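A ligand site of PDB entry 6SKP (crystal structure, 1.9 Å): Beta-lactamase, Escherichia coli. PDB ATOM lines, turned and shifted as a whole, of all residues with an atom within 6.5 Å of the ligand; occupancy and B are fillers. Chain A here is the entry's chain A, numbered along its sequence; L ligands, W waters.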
ATOM      1  N   PRO A  65     -10.814   7.540  28.338  1.00  0.00           N
ATOM      2  CA  PRO A  65     -12.192   7.980  28.642  1.00  0.00           C
ATOM      3  C   PRO A  65     -12.375   9.485  28.723  1.00  0.00           C
ATOM      4  O   PRO A  65     -13.504   9.960  28.495  1.00  0.00           O
ATOM      5  CB  PRO A  65     -12.517   7.305  29.981  1.00  0.00           C
ATOM      6  CG  PRO A  65     -11.198   6.748  30.520  1.00  0.00           C
ATOM      7  CD  PRO A  65     -10.207   6.692  29.389  1.00  0.00           C
ATOM      8  N   ALA A  66     -11.315  10.246  28.983  1.00  0.00           N
ATOM      9  CA  ALA A  66     -11.372  11.698  29.150  1.00  0.00           C
ATOM     10  C   ALA A  66     -12.478  11.963  30.143  1.00  0.00           C
ATOM     11  O   ALA A  66     -12.671  11.183  31.098  1.00  0.00           O
ATOM     12  CB  ALA A  66     -11.623  12.424  27.834  1.00  0.00           C
ATOM     13  N   SER A  67     -13.249  13.039  29.902  1.00  0.00           N
ATOM     14  CA  SER A  67     -14.224  13.463  30.901  1.00  0.00           C
ATOM     15  C   SER A  67     -15.286  12.414  31.228  1.00  0.00           C
ATOM     16  O   SER A  67     -15.969  12.565  32.237  1.00  0.00           O
ATOM     17  CB  SER A  67     -14.990  14.728  30.481  1.00  0.00           C
ATOM     18  OG  SER A  67     -14.152  15.892  30.511  1.00  0.00           O
ATOM     19  N   THR A  68     -15.474  11.379  30.387  1.00  0.00           N
ATOM     20  CA  THR A  68     -16.471  10.370  30.748  1.00  0.00           C
ATOM     21  C   THR A  68     -16.076   9.654  32.027  1.00  0.00           C
ATOM     22  O   THR A  68     -16.927   9.027  32.681  1.00  0.00           O
ATOM     23  CB  THR A  68     -16.695   9.378  29.596  1.00  0.00           C
ATOM     24  OG1 THR A  68     -15.576   8.469  29.470  1.00  0.00           O
ATOM     25  CG2 THR A  68     -16.970  10.164  28.298  1.00  0.00           C
ATOM     26  N   KCX A  70     -15.526  10.897  34.718  1.00  0.00           N
ATOM     27  CA  KCX A  70     -16.186  11.547  35.827  1.00  0.00           C
ATOM     28  CB  KCX A  70     -16.656  12.965  35.419  1.00  0.00           C
ATOM     29  CG  KCX A  70     -15.490  13.943  35.275  1.00  0.00           C
ATOM     30  CD  KCX A  70     -15.871  15.380  34.999  1.00  0.00           C
ATOM     31  CE  KCX A  70     -14.605  16.263  34.952  1.00  0.00           C
ATOM     32  NZ  KCX A  70     -13.649  15.804  33.913  1.00  0.00           N
ATOM     33  C   KCX A  70     -17.357  10.701  36.379  1.00  0.00           C
ATOM     34  O   KCX A  70     -17.762  10.828  37.546  1.00  0.00           O
ATOM     35  CX  KCX A  70     -12.569  15.039  34.191  1.00  0.00           C
ATOM     36  OQ1 KCX A  70     -12.214  14.667  35.324  1.00  0.00           O
ATOM     37  OQ2 KCX A  70     -11.864  14.682  33.242  1.00  0.00           O
ATOM     38  N   MET A  99     -10.263  26.431  32.532  1.00  0.00           N
ATOM     39  CA  MET A  99     -11.417  26.911  31.791  1.00  0.00           C
ATOM     40  C   MET A  99     -12.146  27.854  32.723  1.00  0.00           C
ATOM     41  O   MET A  99     -12.322  27.530  33.908  1.00  0.00           O
ATOM     42  CB  MET A  99     -12.336  25.761  31.385  1.00  0.00           C
ATOM     43  CG  MET A  99     -11.689  24.838  30.364  1.00  0.00           C
ATOM     44  SD  MET A  99     -12.875  23.762  29.559  1.00  0.00           S
ATOM     45  CE  MET A  99     -11.822  22.522  28.864  1.00  0.00           C
ATOM     46  N   GLN A 101     -15.261  28.658  32.881  1.00  0.00           N
ATOM     47  CA  GLN A 101     -16.432  27.957  33.414  1.00  0.00           C
ATOM     48  C   GLN A 101     -16.158  27.164  34.688  1.00  0.00           C
ATOM     49  O   GLN A 101     -17.086  26.848  35.436  1.00  0.00           O
ATOM     50  CB  GLN A 101     -16.970  26.985  32.345  1.00  0.00           C
ATOM     51  CG  GLN A 101     -17.093  27.560  30.920  1.00  0.00           C
ATOM     52  CD  GLN A 101     -15.823  27.402  30.086  1.00  0.00           C
ATOM     53  OE1 GLN A 101     -14.900  28.209  30.180  1.00  0.00           O
ATOM     54  NE2 GLN A 101     -15.774  26.350  29.246  1.00  0.00           N
ATOM     55  N   TRP A 102     -14.908  26.781  34.937  1.00  0.00           N
ATOM     56  CA  TRP A 102     -14.602  26.045  36.144  1.00  0.00           C
ATOM     57  C   TRP A 102     -14.308  26.940  37.359  1.00  0.00           C
ATOM     58  O   TRP A 102     -14.167  26.415  38.470  1.00  0.00           O
ATOM     59  CB  TRP A 102     -13.396  25.121  35.920  1.00  0.00           C
ATOM     60  CG  TRP A 102     -13.526  24.124  34.756  1.00  0.00           C
ATOM     61  CD1 TRP A 102     -14.662  23.724  34.112  1.00  0.00           C
ATOM     62  CD2 TRP A 102     -12.446  23.393  34.170  1.00  0.00           C
ATOM     63  NE1 TRP A 102     -14.333  22.804  33.112  1.00  0.00           N
ATOM     64  CE2 TRP A 102     -12.983  22.604  33.139  1.00  0.00           C
ATOM     65  CE3 TRP A 102     -11.077  23.356  34.406  1.00  0.00           C
ATOM     66  CZ2 TRP A 102     -12.198  21.760  32.363  1.00  0.00           C
ATOM     67  CZ3 TRP A 102     -10.305  22.516  33.633  1.00  0.00           C
ATOM     68  CH2 TRP A 102     -10.856  21.732  32.635  1.00  0.00           C
ATOM     69  N   VAL A 114     -20.168  20.786  33.607  1.00  0.00           N
ATOM     70  CA  VAL A 114     -19.158  21.624  32.989  1.00  0.00           C
ATOM     71  C   VAL A 114     -17.827  20.897  32.871  1.00  0.00           C
ATOM     72  O   VAL A 114     -16.834  21.485  32.423  1.00  0.00           O
ATOM     73  CB  VAL A 114     -18.937  22.966  33.722  1.00  0.00           C
ATOM     74  CG1 VAL A 114     -20.208  23.782  33.793  1.00  0.00           C
ATOM     75  CG2 VAL A 114     -18.310  22.724  35.091  1.00  0.00           C
ATOM     76  N   SER A 115     -17.787  19.619  33.262  1.00  0.00           N
ATOM     77  CA  SER A 115     -16.566  18.805  33.233  1.00  0.00           C
ATOM     78  C   SER A 115     -15.393  19.487  33.921  1.00  0.00           C
ATOM     79  O   SER A 115     -14.300  19.602  33.352  1.00  0.00           O
ATOM     80  CB  SER A 115     -16.169  18.458  31.812  1.00  0.00           C
ATOM     81  OG  SER A 115     -17.073  17.579  31.199  1.00  0.00           O
ATOM     82  N   ALA A 116     -15.621  19.898  35.174  1.00  0.00           N
ATOM     83  CA  ALA A 116     -14.602  20.585  35.972  1.00  0.00           C
ATOM     84  C   ALA A 116     -13.497  19.617  36.417  1.00  0.00           C
ATOM     85  O   ALA A 116     -13.492  19.062  37.529  1.00  0.00           O
ATOM     86  CB  ALA A 116     -15.246  21.307  37.159  1.00  0.00           C
ATOM     87  N   VAL A 117     -12.521  19.482  35.553  1.00  0.00           N
ATOM     88  CA  VAL A 117     -11.405  18.557  35.765  1.00  0.00           C
ATOM     89  C   VAL A 117     -10.777  18.710  37.164  1.00  0.00           C
ATOM     90  O   VAL A 117     -10.485  17.688  37.779  1.00  0.00           O
ATOM     91  CB  VAL A 117     -10.375  18.724  34.657  1.00  0.00           C
ATOM     92  CG1 VAL A 117      -9.072  18.027  34.969  1.00  0.00           C
ATOM     93  CG2 VAL A 117     -10.878  18.180  33.333  1.00  0.00           C
ATOM     94  N   TRP A 154      -6.792   9.117  33.418  1.00  0.00           N
ATOM     95  CA  TRP A 154      -7.905   9.075  32.455  1.00  0.00           C
ATOM     96  C   TRP A 154      -7.834  10.179  31.412  1.00  0.00           C
ATOM     97  O   TRP A 154      -8.671  10.213  30.509  1.00  0.00           O
ATOM     98  CB  TRP A 154      -9.234   9.186  33.189  1.00  0.00           C
ATOM     99  CG  TRP A 154      -9.479  10.576  33.833  1.00  0.00           C
ATOM    100  CD1 TRP A 154     -10.194  11.611  33.331  1.00  0.00           C
ATOM    101  CD2 TRP A 154      -9.045  10.998  35.138  1.00  0.00           C
ATOM    102  NE1 TRP A 154     -10.254  12.647  34.270  1.00  0.00           N
ATOM    103  CE2 TRP A 154      -9.492  12.317  35.350  1.00  0.00           C
ATOM    104  CE3 TRP A 154      -8.299  10.370  36.158  1.00  0.00           C
ATOM    105  CZ2 TRP A 154      -9.245  13.024  36.533  1.00  0.00           C
ATOM    106  CZ3 TRP A 154      -7.997  11.083  37.310  1.00  0.00           C
ATOM    107  CH2 TRP A 154      -8.499  12.380  37.507  1.00  0.00           C
ATOM    108  N   LEU A 155      -6.892  11.095  31.551  1.00  0.00           N
ATOM    109  CA  LEU A 155      -6.710  12.248  30.703  1.00  0.00           C
ATOM    110  C   LEU A 155      -5.537  12.083  29.750  1.00  0.00           C
ATOM    111  O   LEU A 155      -5.625  12.505  28.605  1.00  0.00           O
ATOM    112  CB  LEU A 155      -6.431  13.483  31.563  1.00  0.00           C
ATOM    113  CG  LEU A 155      -7.510  13.959  32.536  1.00  0.00           C
ATOM    114  CD1 LEU A 155      -6.980  15.123  33.398  1.00  0.00           C
ATOM    115  CD2 LEU A 155      -8.785  14.377  31.806  1.00  0.00           C
ATOM    116  N   LYS A 205     -23.090  11.843  29.201  1.00  0.00           N
ATOM    117  CA  LYS A 205     -21.830  12.519  29.550  1.00  0.00           C
ATOM    118  C   LYS A 205     -20.979  12.650  28.300  1.00  0.00           C
ATOM    119  O   LYS A 205     -20.794  11.660  27.582  1.00  0.00           O
ATOM    120  CB  LYS A 205     -21.063  11.737  30.627  1.00  0.00           C
ATOM    121  CG  LYS A 205     -19.704  12.377  31.092  1.00  0.00           C
ATOM    122  CD  LYS A 205     -19.973  13.606  32.031  1.00  0.00           C
ATOM    123  CE  LYS A 205     -18.775  14.574  32.072  1.00  0.00           C
ATOM    124  NZ  LYS A 205     -18.624  15.470  30.913  1.00  0.00           N
ATOM    125  N   THR A 206     -20.434  13.855  28.085  1.00  0.00           N
ATOM    126  CA  THR A 206     -19.571  14.145  26.949  1.00  0.00           C
ATOM    127  C   THR A 206     -18.106  14.066  27.397  1.00  0.00           C
ATOM    128  O   THR A 206     -17.768  14.166  28.582  1.00  0.00           O
ATOM    129  CB  THR A 206     -19.819  15.546  26.349  1.00  0.00           C
ATOM    130  OG1 THR A 206     -19.625  16.527  27.384  1.00  0.00           O
ATOM    131  CG2 THR A 206     -21.213  15.729  25.754  1.00  0.00           C
ATOM    132  N   GLY A 207     -17.209  13.899  26.419  1.00  0.00           N
ATOM    133  CA  GLY A 207     -15.795  13.979  26.710  1.00  0.00           C
ATOM    134  C   GLY A 207     -15.050  14.345  25.454  1.00  0.00           C
ATOM    135  O   GLY A 207     -15.538  14.139  24.335  1.00  0.00           O
ATOM    136  N   PHE A 208     -13.818  14.871  25.639  1.00  0.00           N
ATOM    137  CA  PHE A 208     -12.963  15.358  24.553  1.00  0.00           C
ATOM    138  C   PHE A 208     -11.557  15.287  25.123  1.00  0.00           C
ATOM    139  O   PHE A 208     -11.257  15.996  26.078  1.00  0.00           O
ATOM    140  CB  PHE A 208     -13.360  16.796  24.173  1.00  0.00           C
ATOM    141  CG  PHE A 208     -12.440  17.508  23.189  1.00  0.00           C
ATOM    142  CD1 PHE A 208     -11.928  16.862  22.088  1.00  0.00           C
ATOM    143  CD2 PHE A 208     -12.161  18.883  23.342  1.00  0.00           C
ATOM    144  CE1 PHE A 208     -11.120  17.566  21.144  1.00  0.00           C
ATOM    145  CE2 PHE A 208     -11.364  19.585  22.426  1.00  0.00           C
ATOM    146  CZ  PHE A 208     -10.826  18.908  21.309  1.00  0.00           C
ATOM    147  N   SER A 209     -10.710  14.413  24.555  1.00  0.00           N
ATOM    148  CA  SER A 209      -9.386  14.270  25.158  1.00  0.00           C
ATOM    149  C   SER A 209      -8.435  15.374  24.735  1.00  0.00           C
ATOM    150  O   SER A 209      -7.393  15.544  25.358  1.00  0.00           O
ATOM    151  CB  SER A 209      -8.730  12.937  24.787  1.00  0.00           C
ATOM    152  OG  SER A 209      -8.349  12.961  23.427  1.00  0.00           O
ATOM    153  N   TRP A 221     -16.237  11.915  22.946  1.00  0.00           N
ATOM    154  CA  TRP A 221     -17.185  10.944  23.411  1.00  0.00           C
ATOM    155  C   TRP A 221     -18.541  11.594  23.650  1.00  0.00           C
ATOM    156  O   TRP A 221     -18.620  12.711  24.144  1.00  0.00           O
ATOM    157  CB  TRP A 221     -16.766  10.337  24.752  1.00  0.00           C
ATOM    158  CG  TRP A 221     -15.629   9.357  24.861  1.00  0.00           C
ATOM    159  CD1 TRP A 221     -14.332   9.647  25.163  1.00  0.00           C
ATOM    160  CD2 TRP A 221     -15.732   7.943  24.768  1.00  0.00           C
ATOM    161  NE1 TRP A 221     -13.605   8.452  25.228  1.00  0.00           N
ATOM    162  CE2 TRP A 221     -14.446   7.401  25.009  1.00  0.00           C
ATOM    163  CE3 TRP A 221     -16.787   7.052  24.499  1.00  0.00           C
ATOM    164  CZ2 TRP A 221     -14.190   6.019  24.996  1.00  0.00           C
ATOM    165  CZ3 TRP A 221     -16.533   5.706  24.494  1.00  0.00           C
ATOM    166  CH2 TRP A 221     -15.242   5.188  24.763  1.00  0.00           C
ATOM    167  N   GLU A 244     -10.803  21.062  17.058  1.00  0.00           N
ATOM    168  CA  GLU A 244     -11.924  21.276  17.981  1.00  0.00           C
ATOM    169  C   GLU A 244     -13.173  21.760  17.251  1.00  0.00           C
ATOM    170  O   GLU A 244     -14.277  21.590  17.774  1.00  0.00           O
ATOM    171  CB  GLU A 244     -11.503  22.262  19.084  1.00  0.00           C
ATOM    172  CG  GLU A 244     -12.526  22.368  20.208  1.00  0.00           C
ATOM    173  CD  GLU A 244     -12.026  23.187  21.401  1.00  0.00           C
ATOM    174  OE1 GLU A 244     -10.794  23.259  21.596  1.00  0.00           O
ATOM    175  OE2 GLU A 244     -12.867  23.766  22.137  1.00  0.00           O
ATOM    176  N   LEU A 247     -16.045  19.377  17.032  1.00  0.00           N
ATOM    177  CA  LEU A 247     -16.593  18.822  18.261  1.00  0.00           C
ATOM    178  C   LEU A 247     -18.116  18.674  18.243  1.00  0.00           C
ATOM    179  O   LEU A 247     -18.610  17.665  18.763  1.00  0.00           O
ATOM    180  CB  LEU A 247     -16.146  19.663  19.460  1.00  0.00           C
ATOM    181  CG  LEU A 247     -16.293  18.962  20.815  1.00  0.00           C
ATOM    182  CD1 LEU A 247     -15.508  17.615  20.897  1.00  0.00           C
ATOM    183  CD2 LEU A 247     -15.882  19.858  21.983  1.00  0.00           C
ATOM    184  N   ARG A 250     -19.805  15.182  17.703  1.00  0.00           N
ATOM    185  CA  ARG A 250     -19.946  14.161  18.726  1.00  0.00           C
ATOM    186  C   ARG A 250     -21.389  14.009  19.196  1.00  0.00           C
ATOM    187  O   ARG A 250     -21.774  12.918  19.636  1.00  0.00           O
ATOM    188  CB  ARG A 250     -19.040  14.496  19.901  1.00  0.00           C
ATOM    189  CG  ARG A 250     -19.694  14.214  21.181  1.00  0.00           C
ATOM    190  CD  ARG A 250     -18.929  14.852  22.245  1.00  0.00           C
ATOM    191  NE  ARG A 250     -19.132  16.280  22.402  1.00  0.00           N
ATOM    192  CZ  ARG A 250     -18.431  16.985  23.268  1.00  0.00           C
ATOM    193  NH1 ARG A 250     -17.509  16.347  23.981  1.00  0.00           N
ATOM    194  NH2 ARG A 250     -18.618  18.286  23.421  1.00  0.00           N
HETATM  195  C1  LIG L   1     -13.298  15.895  29.433  1.00  0.00           C
HETATM  196  C2  LIG L   1     -14.534  19.439  27.058  1.00  0.00           C
HETATM  197  C3  LIG L   1     -12.805  17.275  29.167  1.00  0.00           C
HETATM  198  C4  LIG L   1     -13.925  18.335  29.131  1.00  0.00           C
HETATM  199  C5  LIG L   1     -15.399  18.442  27.325  1.00  0.00           C
HETATM  200  O1  LIG L   1     -13.591  15.224  28.431  1.00  0.00           O
HETATM  201  C6  LIG L   1     -11.754  17.580  30.219  1.00  0.00           C
HETATM  202  O2  LIG L   1     -11.164  18.831  29.880  1.00  0.00           O
HETATM  203  C7  LIG L   1     -10.700  16.505  30.381  1.00  0.00           C
HETATM  204  N1  LIG L   1     -15.132  17.799  28.510  1.00  0.00           N
HETATM  205  C8  LIG L   1     -16.525  17.997  26.484  1.00  0.00           C
HETATM  206  O3  LIG L   1     -16.758  18.557  25.418  1.00  0.00           O
HETATM  207  O4  LIG L   1     -17.238  16.979  26.947  1.00  0.00           O
HETATM  208  S1  LIG L   1     -14.646  20.427  25.594  1.00  0.00           S
HETATM  209  C9  LIG L   1     -14.171  22.109  25.993  1.00  0.00           C
HETATM  210  C10 LIG L   1     -13.260  22.699  24.920  1.00  0.00           C
HETATM  211  N2  LIG L   1     -11.948  22.079  24.947  1.00  0.00           N
HETATM  212  C11 LIG L   1     -10.839  22.813  24.726  1.00  0.00           C
HETATM  213  C12 LIG L   1     -13.575  19.509  28.202  1.00  0.00           C
HETATM  214  O   HOH W   1      -8.052  21.786  23.709  1.00  0.00           O
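NZ of KCX 70 sits at hydrogen-bond distance from the side-chain hydroxyl of Ser 67 (3.4 Å). The guanidinium group (NH1) of Arg 250 sits at hydrogen-bond distance from the backbone carbonyl oxygen (O) of Gly 207. The backbone carbonyl oxygen of Gly 207 sits at hydrogen-bond distance from the backbone NH of Trp 221, at 2.7 Å. The backbone carbonyl oxygen (O) of Ser 115 lies close to the indole nitrogen (NE1) of Trp 102 (3.2 Å). OG of Ser 115 sits at hydrogen-bond distance from NZ of Lys 205 (2.6 Å). O of Trp 154 is in hydrogen-bond range of N of Ala 66 (3.1 Å). OQ2 of KCX 70 lies within hydrogen-bond range of the indole nitrogen (NE1) of Trp 154, 2.8 Å away. The indole nitrogen of Trp 102 is in hydrogen-bond range of the backbone carbonyl oxygen of Val 114.
Residues that only touch the ligand: Leu 155 (3.2 Å), Val 117 (3.3 Å), Ala 66 (3.5 Å), Met 99 (3.5 Å), KCX 70 (3.6 Å), Leu 247 (3.8 Å) and Trp 102 (3.98 Å). Hydrophobic or aromatic side chains that line the ligand: Ala 66, Met 99, Trp 102, Val 117, Leu 155, Phe 208 and Leu 247.
The backbone NH (N) of Ser 67 lies close to an oxygen (O1) of the ligand (2.7 Å). The side-chain hydroxyl of Ser 67 is covalently linked to a carbon (C1) of the ligand, 1.4 Å away. An oxygen (O4) of the ligand sits at hydrogen-bond distance from the side-chain hydroxyl of Thr 206, at 2.5 Å. The guanidinium group (NH1) of Arg 250 lies within salt-bridge range of an oxygen (O3) of the ligand. N of Phe 208 lies within hydrogen-bond range of O1 of the ligand, at 2.8 Å. OE2 of Glu 244 lies within salt-bridge range of N2 of the ligand (3.4 Å). O4 of the ligand lies within hydrogen-bond range of N of Gly 207, at 3.1 Å. The side-chain hydroxyl (OG) of Ser 115 is in hydrogen-bond range of a nitrogen (N1) of the ligand (3.3 Å).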
